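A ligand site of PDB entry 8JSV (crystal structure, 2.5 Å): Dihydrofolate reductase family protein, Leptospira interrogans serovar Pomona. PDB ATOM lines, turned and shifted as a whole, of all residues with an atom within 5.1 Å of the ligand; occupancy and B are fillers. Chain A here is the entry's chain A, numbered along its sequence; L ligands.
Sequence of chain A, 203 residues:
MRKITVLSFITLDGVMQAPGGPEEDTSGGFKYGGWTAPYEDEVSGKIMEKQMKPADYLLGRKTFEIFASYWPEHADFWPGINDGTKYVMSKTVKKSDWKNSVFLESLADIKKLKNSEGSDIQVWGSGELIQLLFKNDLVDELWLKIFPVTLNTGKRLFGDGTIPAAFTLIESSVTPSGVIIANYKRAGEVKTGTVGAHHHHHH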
ATOM      1  N   LEU A   7      -6.609   6.776 -16.488  1.00  0.00           N
ATOM      2  CA  LEU A   7      -6.591   8.226 -16.591  1.00  0.00           C
ATOM      3  C   LEU A   7      -7.519   8.623 -17.719  1.00  0.00           C
ATOM      4  O   LEU A   7      -7.445   8.054 -18.809  1.00  0.00           O
ATOM      5  CB  LEU A   7      -5.178   8.737 -16.839  1.00  0.00           C
ATOM      6  CG  LEU A   7      -4.187   8.383 -15.730  1.00  0.00           C
ATOM      7  CD1 LEU A   7      -3.432   7.081 -16.023  1.00  0.00           C
ATOM      8  CD2 LEU A   7      -3.213   9.515 -15.500  1.00  0.00           C
ATOM      9  N   SER A   8      -8.408   9.575 -17.463  1.00  0.00           N
ATOM     10  CA  SER A   8      -9.425   9.827 -18.473  1.00  0.00           C
ATOM     11  C   SER A   8      -9.870  11.287 -18.447  1.00  0.00           C
ATOM     12  O   SER A   8      -9.918  11.920 -17.380  1.00  0.00           O
ATOM     13  CB  SER A   8     -10.632   8.881 -18.274  1.00  0.00           C
ATOM     14  OG  SER A   8     -11.229   8.501 -19.506  1.00  0.00           O
ATOM     15  N   PHE A   9     -10.171  11.807 -19.620  1.00  0.00           N
ATOM     16  CA  PHE A   9     -10.815  13.105 -19.775  1.00  0.00           C
ATOM     17  C   PHE A   9     -12.298  12.857 -20.018  1.00  0.00           C
ATOM     18  O   PHE A   9     -12.654  12.173 -20.987  1.00  0.00           O
ATOM     19  CB  PHE A   9     -10.240  13.892 -20.950  1.00  0.00           C
ATOM     20  CG  PHE A   9      -8.747  14.123 -20.907  1.00  0.00           C
ATOM     21  CD1 PHE A   9      -8.026  14.064 -19.743  1.00  0.00           C
ATOM     22  CD2 PHE A   9      -8.079  14.481 -22.079  1.00  0.00           C
ATOM     23  CE1 PHE A   9      -6.653  14.304 -19.750  1.00  0.00           C
ATOM     24  CE2 PHE A   9      -6.732  14.738 -22.089  1.00  0.00           C
ATOM     25  CZ  PHE A   9      -6.009  14.648 -20.919  1.00  0.00           C
ATOM     26  N   ILE A  10     -13.172  13.409 -19.174  1.00  0.00           N
ATOM     27  CA  ILE A  10     -14.597  13.189 -19.413  1.00  0.00           C
ATOM     28  C   ILE A  10     -15.367  14.499 -19.324  1.00  0.00           C
ATOM     29  O   ILE A  10     -14.981  15.449 -18.635  1.00  0.00           O
ATOM     30  CB  ILE A  10     -15.247  12.147 -18.476  1.00  0.00           C
ATOM     31  CG1 ILE A  10     -14.965  12.478 -17.016  1.00  0.00           C
ATOM     32  CG2 ILE A  10     -14.776  10.731 -18.805  1.00  0.00           C
ATOM     33  CD1 ILE A  10     -15.327  11.354 -16.091  1.00  0.00           C
ATOM     34  N   MET A  16     -16.257  10.261 -23.223  1.00  0.00           N
ATOM     35  CA  MET A  16     -14.807  10.260 -23.251  1.00  0.00           C
ATOM     36  C   MET A  16     -14.237  10.226 -24.698  1.00  0.00           C
ATOM     37  O   MET A  16     -13.037  10.408 -24.915  1.00  0.00           O
ATOM     38  CB  MET A  16     -14.303   9.087 -22.414  1.00  0.00           C
ATOM     39  CG  MET A  16     -14.765   7.744 -22.951  1.00  0.00           C
ATOM     40  SD  MET A  16     -13.390   6.893 -24.087  1.00  0.00           S
ATOM     41  CE  MET A  16     -12.106   6.636 -22.624  1.00  0.00           C
ATOM     42  N   GLN A  17     -15.138  10.061 -25.667  1.00  0.00           N
ATOM     43  CA  GLN A  17     -14.729   9.918 -27.071  1.00  0.00           C
ATOM     44  C   GLN A  17     -14.055  11.185 -27.591  1.00  0.00           C
ATOM     45  O   GLN A  17     -14.554  12.302 -27.402  1.00  0.00           O
ATOM     46  CB  GLN A  17     -15.952   9.582 -27.913  1.00  0.00           C
ATOM     47  CG  GLN A  17     -15.714   9.402 -29.399  1.00  0.00           C
ATOM     48  CD  GLN A  17     -16.923   8.794 -30.051  1.00  0.00           C
ATOM     49  OE1 GLN A  17     -17.798   8.299 -29.338  1.00  0.00           O
ATOM     50  NE2 GLN A  17     -16.992   8.811 -31.383  1.00  0.00           N
ATOM     51  N   ALA A  18     -12.915  10.985 -28.268  1.00  0.00           N
ATOM     52  CA  ALA A  18     -12.284  11.999 -29.098  1.00  0.00           C
ATOM     53  C   ALA A  18     -12.012  13.338 -28.374  1.00  0.00           C
ATOM     54  O   ALA A  18     -12.420  14.388 -28.835  1.00  0.00           O
ATOM     55  CB  ALA A  18     -13.133  12.243 -30.333  1.00  0.00           C
ATOM     56  N   PRO A  19     -11.298  13.296 -27.243  1.00  0.00           N
ATOM     57  CA  PRO A  19     -10.986  14.581 -26.591  1.00  0.00           C
ATOM     58  C   PRO A  19     -10.185  15.523 -27.473  1.00  0.00           C
ATOM     59  O   PRO A  19     -10.484  16.728 -27.506  1.00  0.00           O
ATOM     60  CB  PRO A  19     -10.181  14.148 -25.362  1.00  0.00           C
ATOM     61  CG  PRO A  19      -9.611  12.837 -25.722  1.00  0.00           C
ATOM     62  CD  PRO A  19     -10.645  12.171 -26.580  1.00  0.00           C
ATOM     63  N   GLU A  24     -10.289  12.541 -34.238  1.00  0.00           N
ATOM     64  CA  GLU A  24      -9.678  11.521 -33.400  1.00  0.00           C
ATOM     65  C   GLU A  24     -10.507  10.247 -33.353  1.00  0.00           C
ATOM     66  O   GLU A  24      -9.937   9.151 -33.273  1.00  0.00           O
ATOM     67  CB  GLU A  24      -9.456  12.065 -31.997  1.00  0.00           C
ATOM     68  CG  GLU A  24      -8.814  11.053 -31.069  1.00  0.00           C
ATOM     69  CD  GLU A  24      -8.526  11.616 -29.701  1.00  0.00           C
ATOM     70  OE1 GLU A  24      -8.191  12.811 -29.634  1.00  0.00           O
ATOM     71  OE2 GLU A  24      -8.629  10.848 -28.711  1.00  0.00           O
ATOM     72  N   ASP A  25     -11.835  10.362 -33.399  1.00  0.00           N
ATOM     73  CA  ASP A  25     -12.703   9.176 -33.438  1.00  0.00           C
ATOM     74  C   ASP A  25     -14.066   9.579 -33.960  1.00  0.00           C
ATOM     75  O   ASP A  25     -14.849  10.204 -33.232  1.00  0.00           O
ATOM     76  CB  ASP A  25     -12.821   8.557 -32.047  1.00  0.00           C
ATOM     77  CG  ASP A  25     -13.731   7.331 -32.018  1.00  0.00           C
ATOM     78  OD1 ASP A  25     -14.306   6.976 -33.082  1.00  0.00           O
ATOM     79  OD2 ASP A  25     -13.869   6.728 -30.914  1.00  0.00           O
ATOM     80  N   TRP A  35     -13.410  18.507 -28.007  1.00  0.00           N
ATOM     81  CA  TRP A  35     -14.096  19.270 -26.960  1.00  0.00           C
ATOM     82  C   TRP A  35     -13.176  19.573 -25.782  1.00  0.00           C
ATOM     83  O   TRP A  35     -13.447  20.497 -25.015  1.00  0.00           O
ATOM     84  CB  TRP A  35     -15.328  18.505 -26.487  1.00  0.00           C
ATOM     85  CG  TRP A  35     -15.036  17.084 -26.152  1.00  0.00           C
ATOM     86  CD1 TRP A  35     -15.092  15.995 -26.995  1.00  0.00           C
ATOM     87  CD2 TRP A  35     -14.593  16.607 -24.898  1.00  0.00           C
ATOM     88  NE1 TRP A  35     -14.708  14.865 -26.316  1.00  0.00           N
ATOM     89  CE2 TRP A  35     -14.398  15.211 -25.022  1.00  0.00           C
ATOM     90  CE3 TRP A  35     -14.353  17.212 -23.659  1.00  0.00           C
ATOM     91  CZ2 TRP A  35     -13.995  14.417 -23.956  1.00  0.00           C
ATOM     92  CZ3 TRP A  35     -13.948  16.426 -22.604  1.00  0.00           C
ATOM     93  CH2 TRP A  35     -13.781  15.041 -22.760  1.00  0.00           C
ATOM     94  N   GLY A  60      -6.127  -0.467 -25.409  1.00  0.00           N
ATOM     95  CA  GLY A  60      -6.861  -1.147 -26.464  1.00  0.00           C
ATOM     96  C   GLY A  60      -6.241  -0.874 -27.824  1.00  0.00           C
ATOM     97  O   GLY A  60      -5.602   0.143 -28.045  1.00  0.00           O
ATOM     98  N   ARG A  61      -6.405  -1.827 -28.750  1.00  0.00           N
ATOM     99  CA  ARG A  61      -5.692  -1.675 -30.019  1.00  0.00           C
ATOM    100  C   ARG A  61      -5.972  -0.321 -30.648  1.00  0.00           C
ATOM    101  O   ARG A  61      -5.069   0.309 -31.212  1.00  0.00           O
ATOM    102  CB  ARG A  61      -6.054  -2.770 -31.018  1.00  0.00           C
ATOM    103  CG  ARG A  61      -6.123  -2.159 -32.413  1.00  0.00           C
ATOM    104  CD  ARG A  61      -6.388  -3.072 -33.487  1.00  0.00           C
ATOM    105  NE  ARG A  61      -7.822  -3.283 -33.687  1.00  0.00           N
ATOM    106  CZ  ARG A  61      -8.624  -2.438 -34.307  1.00  0.00           C
ATOM    107  NH1 ARG A  61      -8.232  -1.212 -34.632  1.00  0.00           N
ATOM    108  NH2 ARG A  61      -9.863  -2.833 -34.631  1.00  0.00           N
ATOM    109  N   LYS A  62      -7.218   0.155 -30.555  1.00  0.00           N
ATOM    110  CA  LYS A  62      -7.576   1.394 -31.233  1.00  0.00           C
ATOM    111  C   LYS A  62      -6.813   2.577 -30.654  1.00  0.00           C
ATOM    112  O   LYS A  62      -6.269   3.410 -31.389  1.00  0.00           O
ATOM    113  CB  LYS A  62      -9.075   1.622 -31.174  1.00  0.00           C
ATOM    114  CG  LYS A  62      -9.876   0.716 -32.116  1.00  0.00           C
ATOM    115  CD  LYS A  62     -11.329   0.578 -31.648  1.00  0.00           C
ATOM    116  CE  LYS A  62     -12.224   0.000 -32.697  1.00  0.00           C
ATOM    117  NZ  LYS A  62     -13.577  -0.272 -32.146  1.00  0.00           N
ATOM    118  N   THR A  63      -6.762   2.660 -29.318  1.00  0.00           N
ATOM    119  CA  THR A  63      -5.998   3.727 -28.688  1.00  0.00           C
ATOM    120  C   THR A  63      -4.512   3.553 -28.929  1.00  0.00           C
ATOM    121  O   THR A  63      -3.778   4.544 -29.107  1.00  0.00           O
ATOM    122  CB  THR A  63      -6.332   3.762 -27.205  1.00  0.00           C
ATOM    123  OG1 THR A  63      -7.724   4.061 -27.069  1.00  0.00           O
ATOM    124  CG2 THR A  63      -5.529   4.827 -26.473  1.00  0.00           C
ATOM    125  N   ILE A  66      -3.987   4.987 -32.431  1.00  0.00           N
ATOM    126  CA  ILE A  66      -4.021   6.448 -32.372  1.00  0.00           C
ATOM    127  C   ILE A  66      -2.709   7.002 -31.824  1.00  0.00           C
ATOM    128  O   ILE A  66      -2.197   8.025 -32.298  1.00  0.00           O
ATOM    129  CB  ILE A  66      -5.213   6.922 -31.519  1.00  0.00           C
ATOM    130  CG1 ILE A  66      -6.533   6.537 -32.188  1.00  0.00           C
ATOM    131  CG2 ILE A  66      -5.114   8.437 -31.269  1.00  0.00           C
ATOM    132  CD1 ILE A  66      -7.750   6.738 -31.316  1.00  0.00           C
ATOM    133  N   PHE A  67      -2.149   6.340 -30.804  1.00  0.00           N
ATOM    134  CA  PHE A  67      -0.902   6.841 -30.226  1.00  0.00           C
ATOM    135  C   PHE A  67       0.289   6.615 -31.153  1.00  0.00           C
ATOM    136  O   PHE A  67       1.123   7.504 -31.356  1.00  0.00           O
ATOM    137  CB  PHE A  67      -0.665   6.195 -28.858  1.00  0.00           C
ATOM    138  CG  PHE A  67      -1.372   6.876 -27.715  1.00  0.00           C
ATOM    139  CD1 PHE A  67      -2.186   7.972 -27.943  1.00  0.00           C
ATOM    140  CD2 PHE A  67      -1.248   6.399 -26.425  1.00  0.00           C
ATOM    141  CE1 PHE A  67      -2.843   8.594 -26.882  1.00  0.00           C
ATOM    142  CE2 PHE A  67      -1.896   7.019 -25.364  1.00  0.00           C
ATOM    143  CZ  PHE A  67      -2.697   8.121 -25.603  1.00  0.00           C
ATOM    144  N   MET A  89      -4.025  -4.816 -25.964  1.00  0.00           N
ATOM    145  CA  MET A  89      -4.999  -5.893 -26.061  1.00  0.00           C
ATOM    146  C   MET A  89      -5.503  -5.986 -27.487  1.00  0.00           C
ATOM    147  O   MET A  89      -6.076  -5.031 -28.000  1.00  0.00           O
ATOM    148  CB  MET A  89      -6.141  -5.626 -25.071  1.00  0.00           C
ATOM    149  CG  MET A  89      -7.322  -6.613 -25.068  1.00  0.00           C
ATOM    150  SD  MET A  89      -6.893  -8.358 -24.262  1.00  0.00           S
ATOM    151  CE  MET A  89      -5.358  -7.818 -23.258  1.00  0.00           C
ATOM    152  N   SER A  90      -5.295  -7.118 -28.156  1.00  0.00           N
ATOM    153  CA  SER A  90      -5.759  -7.170 -29.529  1.00  0.00           C
ATOM    154  C   SER A  90      -5.763  -8.615 -30.016  1.00  0.00           C
ATOM    155  O   SER A  90      -4.915  -9.417 -29.617  1.00  0.00           O
ATOM    156  CB  SER A  90      -4.877  -6.317 -30.447  1.00  0.00           C
ATOM    157  OG  SER A  90      -5.084  -6.626 -31.800  1.00  0.00           O
ATOM    158  N   LYS A  91      -6.720  -8.917 -30.889  1.00  0.00           N
ATOM    159  CA  LYS A  91      -6.755 -10.170 -31.633  1.00  0.00           C
ATOM    160  C   LYS A  91      -6.323 -10.006 -33.092  1.00  0.00           C
ATOM    161  O   LYS A  91      -6.001 -11.006 -33.745  1.00  0.00           O
ATOM    162  CB  LYS A  91      -8.157 -10.787 -31.610  1.00  0.00           C
ATOM    163  CG  LYS A  91      -8.714 -11.092 -30.225  1.00  0.00           C
ATOM    164  CD  LYS A  91      -8.055 -12.321 -29.605  1.00  0.00           C
ATOM    165  CE  LYS A  91      -8.758 -12.776 -28.324  1.00  0.00           C
ATOM    166  NZ  LYS A  91      -7.946 -13.733 -27.501  1.00  0.00           N
ATOM    167  N   THR A  92      -6.316  -8.776 -33.623  1.00  0.00           N
ATOM    168  CA  THR A  92      -6.026  -8.559 -35.038  1.00  0.00           C
ATOM    169  C   THR A  92      -4.633  -8.003 -35.294  1.00  0.00           C
ATOM    170  O   THR A  92      -4.223  -7.906 -36.466  1.00  0.00           O
ATOM    171  CB  THR A  92      -7.045  -7.589 -35.666  1.00  0.00           C
ATOM    172  OG1 THR A  92      -6.963  -6.320 -35.007  1.00  0.00           O
ATOM    173  CG2 THR A  92      -8.492  -8.130 -35.574  1.00  0.00           C
ATOM    174  N   VAL A  93      -3.899  -7.628 -34.257  1.00  0.00           N
ATOM    175  CA  VAL A  93      -2.567  -7.058 -34.403  1.00  0.00           C
ATOM    176  C   VAL A  93      -1.626  -7.858 -33.518  1.00  0.00           C
ATOM    177  O   VAL A  93      -1.940  -8.112 -32.340  1.00  0.00           O
ATOM    178  CB  VAL A  93      -2.527  -5.560 -34.037  1.00  0.00           C
ATOM    179  CG1 VAL A  93      -1.145  -5.001 -34.233  1.00  0.00           C
ATOM    180  CG2 VAL A  93      -3.532  -4.812 -34.891  1.00  0.00           C
ATOM    181  N   GLU A 105      -3.858 -11.064 -25.570  1.00  0.00           N
ATOM    182  CA  GLU A 105      -5.098 -11.453 -26.209  1.00  0.00           C
ATOM    183  C   GLU A 105      -6.243 -11.811 -25.271  1.00  0.00           C
ATOM    184  O   GLU A 105      -7.382 -11.934 -25.746  1.00  0.00           O
ATOM    185  CB  GLU A 105      -4.860 -12.661 -27.139  1.00  0.00           C
ATOM    186  CG  GLU A 105      -4.075 -12.335 -28.389  1.00  0.00           C
ATOM    187  CD  GLU A 105      -3.846 -13.570 -29.253  1.00  0.00           C
ATOM    188  OE1 GLU A 105      -2.907 -14.346 -28.931  1.00  0.00           O
ATOM    189  OE2 GLU A 105      -4.593 -13.776 -30.238  1.00  0.00           O
ATOM    190  N   TRP A 124      -4.533   4.687 -20.699  1.00  0.00           N
ATOM    191  CA  TRP A 124      -5.066   5.884 -21.326  1.00  0.00           C
ATOM    192  C   TRP A 124      -6.063   5.484 -22.395  1.00  0.00           C
ATOM    193  O   TRP A 124      -6.007   4.370 -22.931  1.00  0.00           O
ATOM    194  CB  TRP A 124      -3.957   6.723 -21.962  1.00  0.00           C
ATOM    195  CG  TRP A 124      -2.934   7.222 -21.003  1.00  0.00           C
ATOM    196  CD1 TRP A 124      -1.886   6.535 -20.506  1.00  0.00           C
ATOM    197  CD2 TRP A 124      -2.850   8.534 -20.453  1.00  0.00           C
ATOM    198  NE1 TRP A 124      -1.140   7.329 -19.675  1.00  0.00           N
ATOM    199  CE2 TRP A 124      -1.730   8.569 -19.617  1.00  0.00           C
ATOM    200  CE3 TRP A 124      -3.630   9.692 -20.581  1.00  0.00           C
ATOM    201  CZ2 TRP A 124      -1.365   9.695 -18.908  1.00  0.00           C
ATOM    202  CZ3 TRP A 124      -3.268  10.807 -19.880  1.00  0.00           C
ATOM    203  CH2 TRP A 124      -2.145  10.810 -19.049  1.00  0.00           C
ATOM    204  N   GLY A 125      -6.966   6.408 -22.712  1.00  0.00           N
ATOM    205  CA  GLY A 125      -8.043   6.116 -23.636  1.00  0.00           C
ATOM    206  C   GLY A 125      -8.641   4.759 -23.335  1.00  0.00           C
ATOM    207  O   GLY A 125      -8.869   4.428 -22.176  1.00  0.00           O
ATOM    208  N   SER A 126      -8.833   3.939 -24.375  1.00  0.00           N
ATOM    209  CA  SER A 126      -9.174   2.522 -24.232  1.00  0.00           C
ATOM    210  C   SER A 126     -10.511   2.330 -23.502  1.00  0.00           C
ATOM    211  O   SER A 126     -10.610   1.625 -22.503  1.00  0.00           O
ATOM    212  CB  SER A 126      -8.062   1.736 -23.505  1.00  0.00           C
ATOM    213  OG  SER A 126      -6.748   2.120 -23.892  1.00  0.00           O
ATOM    214  N   GLY A 127     -11.551   2.966 -24.041  1.00  0.00           N
ATOM    215  CA  GLY A 127     -12.857   2.852 -23.417  1.00  0.00           C
ATOM    216  C   GLY A 127     -13.345   1.410 -23.378  1.00  0.00           C
ATOM    217  O   GLY A 127     -13.757   0.906 -22.327  1.00  0.00           O
ATOM    218  N   GLU A 128     -13.276   0.726 -24.528  1.00  0.00           N
ATOM    219  CA  GLU A 128     -13.758  -0.650 -24.582  1.00  0.00           C
ATOM    220  C   GLU A 128     -12.949  -1.572 -23.684  1.00  0.00           C
ATOM    221  O   GLU A 128     -13.528  -2.425 -22.995  1.00  0.00           O
ATOM    222  CB  GLU A 128     -13.720  -1.148 -26.018  1.00  0.00           C
ATOM    223  CG  GLU A 128     -14.229  -2.559 -26.126  1.00  0.00           C
ATOM    224  CD  GLU A 128     -14.420  -2.981 -27.562  1.00  0.00           C
ATOM    225  OE1 GLU A 128     -13.927  -2.251 -28.471  1.00  0.00           O
ATOM    226  OE2 GLU A 128     -15.067  -4.033 -27.781  1.00  0.00           O
ATOM    227  N   LEU A 129     -11.623  -1.442 -23.671  1.00  0.00           N
ATOM    228  CA  LEU A 129     -10.813  -2.272 -22.779  1.00  0.00           C
ATOM    229  C   LEU A 129     -11.086  -1.942 -21.319  1.00  0.00           C
ATOM    230  O   LEU A 129     -11.074  -2.843 -20.450  1.00  0.00           O
ATOM    231  CB  LEU A 129      -9.315  -2.101 -23.061  1.00  0.00           C
ATOM    232  CG  LEU A 129      -8.465  -2.975 -22.131  1.00  0.00           C
ATOM    233  CD1 LEU A 129      -8.658  -4.462 -22.466  1.00  0.00           C
ATOM    234  CD2 LEU A 129      -6.996  -2.589 -22.126  1.00  0.00           C
ATOM    235  N   LEU A 132     -13.797  -4.018 -19.734  1.00  0.00           N
ATOM    236  CA  LEU A 132     -13.343  -5.298 -19.213  1.00  0.00           C
ATOM    237  C   LEU A 132     -12.523  -5.141 -17.936  1.00  0.00           C
ATOM    238  O   LEU A 132     -12.636  -5.960 -17.008  1.00  0.00           O
ATOM    239  CB  LEU A 132     -12.520  -6.004 -20.283  1.00  0.00           C
ATOM    240  CG  LEU A 132     -12.014  -7.379 -19.868  1.00  0.00           C
ATOM    241  CD1 LEU A 132     -12.693  -8.451 -20.702  1.00  0.00           C
ATOM    242  CD2 LEU A 132     -10.503  -7.396 -20.016  1.00  0.00           C
ATOM    243  N   LYS A 155     -18.813   7.733 -26.833  1.00  0.00           N
ATOM    244  CA  LYS A 155     -18.356   6.580 -26.009  1.00  0.00           C
ATOM    245  C   LYS A 155     -18.211   7.065 -24.574  1.00  0.00           C
ATOM    246  O   LYS A 155     -17.835   8.231 -24.380  1.00  0.00           O
ATOM    247  CB  LYS A 155     -17.078   5.978 -26.588  1.00  0.00           C
ATOM    248  CG  LYS A 155     -17.221   5.289 -27.936  1.00  0.00           C
ATOM    249  CD  LYS A 155     -15.913   5.141 -28.677  1.00  0.00           C
ATOM    250  CE  LYS A 155     -16.034   4.299 -29.917  1.00  0.00           C
ATOM    251  NZ  LYS A 155     -14.716   4.073 -30.553  1.00  0.00           N
HETATM  252  P1  LIG L   1     -10.012   0.673 -27.557  1.00  0.00           P
HETATM  253  O1  LIG L   1     -10.434   0.238 -26.193  1.00  0.00           O
HETATM  254  O2  LIG L   1      -8.943   1.712 -27.485  1.00  0.00           O
HETATM  255  O3  LIG L   1      -9.468  -0.618 -28.366  1.00  0.00           O
HETATM  256  C1  LIG L   1     -10.457  -1.453 -28.881  1.00  0.00           C
HETATM  257  C2  LIG L   1      -9.726  -2.707 -29.405  1.00  0.00           C
HETATM  258  O4  LIG L   1      -8.935  -3.136 -28.461  1.00  0.00           O
HETATM  259  C3  LIG L   1     -10.729  -3.830 -29.625  1.00  0.00           C
HETATM  260  O5  LIG L   1     -11.194  -3.789 -30.893  1.00  0.00           O
HETATM  261  C4  LIG L   1      -9.818  -5.029 -29.371  1.00  0.00           C
HETATM  262  O6  LIG L   1      -8.751  -5.098 -30.405  1.00  0.00           O
HETATM  263  C5  LIG L   1      -9.259  -4.691 -28.253  1.00  0.00           C
HETATM  264  N1  LIG L   1     -10.140  -4.828 -27.126  1.00  0.00           N
HETATM  265  C6  LIG L   1     -10.711  -3.875 -26.378  1.00  0.00           C
HETATM  266  N2  LIG L   1     -11.440  -4.469 -25.437  1.00  0.00           N
HETATM  267  C7  LIG L   1     -11.307  -5.782 -25.585  1.00  0.00           C
HETATM  268  C8  LIG L   1     -11.841  -6.833 -24.892  1.00  0.00           C
HETATM  269  N3  LIG L   1     -12.711  -6.575 -23.764  1.00  0.00           N
HETATM  270  N4  LIG L   1     -11.553  -8.073 -25.239  1.00  0.00           N
HETATM  271  C9  LIG L   1     -10.741  -8.304 -26.300  1.00  0.00           C
HETATM  272  N5  LIG L   1     -10.221  -7.268 -26.979  1.00  0.00           N
HETATM  273  C10 LIG L   1     -10.514  -6.005 -26.627  1.00  0.00           C
HETATM  274  O7  LIG L   1     -11.304   1.162 -28.441  1.00  0.00           O
HETATM  275  P2  LIG L   1     -12.206   2.495 -28.170  1.00  0.00           P
HETATM  276  O8  LIG L   1     -12.277   2.725 -26.696  1.00  0.00           O
HETATM  277  O9  LIG L   1     -13.567   2.255 -28.722  1.00  0.00           O
HETATM  278  O10 LIG L   1     -11.514   3.772 -28.905  1.00  0.00           O
HETATM  279  C11 LIG L   1     -10.665   4.563 -28.126  1.00  0.00           C
HETATM  280  C12 LIG L   1     -11.456   5.781 -27.594  1.00  0.00           C
HETATM  281  O11 LIG L   1     -10.829   6.310 -26.592  1.00  0.00           O
HETATM  282  C13 LIG L   1     -11.474   6.850 -28.696  1.00  0.00           C
HETATM  283  O12 LIG L   1     -12.692   7.429 -28.744  1.00  0.00           O
HETATM  284  C14 LIG L   1     -10.434   7.855 -28.212  1.00  0.00           C
HETATM  285  O13 LIG L   1     -10.701   9.173 -28.855  1.00  0.00           O
HETATM  286  C15 LIG L   1     -10.714   7.879 -26.952  1.00  0.00           C
HETATM  287  N6  LIG L   1      -9.686   8.470 -26.171  1.00  0.00           N
HETATM  288  C16 LIG L   1     -10.035   9.055 -25.018  1.00  0.00           C
HETATM  289  C17 LIG L   1      -9.080   9.647 -24.217  1.00  0.00           C
HETATM  290  C18 LIG L   1      -9.527  10.311 -22.933  1.00  0.00           C
HETATM  291  O14 LIG L   1      -8.763  10.493 -22.056  1.00  0.00           O
HETATM  292  N7  LIG L   1     -10.914  10.714 -22.795  1.00  0.00           N
HETATM  293  C19 LIG L   1      -7.782   9.620 -24.592  1.00  0.00           C
HETATM  294  C20 LIG L   1      -7.425   9.023 -25.743  1.00  0.00           C
HETATM  295  C21 LIG L   1      -8.390   8.433 -26.545  1.00  0.00           C
HETATM  296  P3  LIG L   1      -8.925  -6.000 -31.756  1.00  0.00           P
HETATM  297  O15 LIG L   1      -7.638  -5.979 -32.516  1.00  0.00           O
HETATM  298  O16 LIG L   1      -9.262  -7.419 -31.389  1.00  0.00           O
HETATM  299  O17 LIG L   1     -10.007  -5.445 -32.625  1.00  0.00           O
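The backbone carbonyl oxygen (O) of Met 16 sits at hydrogen-bond distance from a nitrogen (N7) of the ligand (3.0 Å).
The backbone carbonyl oxygen (O) of Phe 9 is in hydrogen-bond range of a nitrogen (N7) of the ligand (2.9 Å).
An oxygen (O13) of the ligand lies within hydrogen-bond range of the backbone NH (N) of Ala 18, at 2.9 Å.
N of Arg 61 sits at hydrogen-bond distance from O4 of the ligand, 2.9 Å away.
The side-chain hydroxyl (OG) of Ser 90 is in hydrogen-bond range of an oxygen (O15) of the ligand (2.7 Å).
O15 of the ligand lies within salt-bridge range of NE of Arg 61 (2.9 Å).
An oxygen (O3) of the ligand lies within hydrogen-bond range of the backbone NH (N) of Lys 62, 3.2 Å away.
N of Gly 127 sits at hydrogen-bond distance from O8 of the ligand (2.8 Å).
The side-chain amino group of Lys 155 lies within salt-bridge range of an oxygen (O9) of the ligand, at 2.8 Å.
The backbone NH (N) of Leu 129 sits at hydrogen-bond distance from an oxygen (O1) of the ligand (3.3 Å).
O16 of the ligand lies within hydrogen-bond range of N of Lys 91 (3.0 Å).
O14 of the ligand sits at hydrogen-bond distance from N of Phe 9 (3.1 Å).
O13 of the ligand lies within hydrogen-bond range of OE2 of Glu 24 (2.7 Å).
The backbone NH (N) of Glu 128 lies within hydrogen-bond range of an oxygen (O8) of the ligand, at 3.1 Å.
The side-chain hydroxyl (OG1) of Thr 92 sits at hydrogen-bond distance from an oxygen (O15) of the ligand, at 2.6 Å.
The backbone NH (N) of Thr 92 sits at hydrogen-bond distance from an oxygen (O15) of the ligand (3.3 Å).
The side-chain carboxylate of Asp 25 lies within hydrogen-bond range of an oxygen (O12) of the ligand (2.6 Å).
O2 of the ligand sits at hydrogen-bond distance from N of Thr 63 (3.0 Å).
An oxygen (O2) of the ligand lies within hydrogen-bond range of the side-chain hydroxyl (OG1) of Thr 63 (2.7 Å).
The backbone NH of Ser 126 lies within hydrogen-bond range of the side-chain hydroxyl of Thr 63 (2.9 Å).
O of Gln 17 lies within hydrogen-bond range of NE1 of Trp 35 (2.8 Å).
NE2 of Gln 17 is in hydrogen-bond range of O of Asp 25.
OG of Ser 126 is in hydrogen-bond range of N of Gly 60, 3.1 Å away.
The backbone carbonyl oxygen (O) of Trp 124 is in hydrogen-bond range of the side-chain hydroxyl (OG) of Ser 126.
The side-chain carboxylate (OD2) of Asp 25 lies within salt-bridge range of the side-chain amino group (NZ) of Lys 155 (2.8 Å).
N of Trp 35 lies within hydrogen-bond range of O of Pro 19 (3.5 Å).
The side-chain hydroxyl of Thr 92 is in hydrogen-bond range of the guanidinium group of Arg 61, 3.4 Å away.
An oxygen (O4) of the ligand lies close to the backbone carbonyl oxygen (O) of Met 89 (3.5 Å).
Residues that only touch the ligand: Ser 8 (3.7 Å), Gln 17 (3.6 Å), Pro 19 (3.5 Å), Gly 60 (3.3 Å), Gly 125 (3.6 Å), Ser 126 (3.3 Å) and Leu 132 (3.5 Å).
Of the 31 residues printed, 23 come within 4 Å of the ligand.
The nearest printed residue that does not touch the ligand is Ile 66 (4.3 Å).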
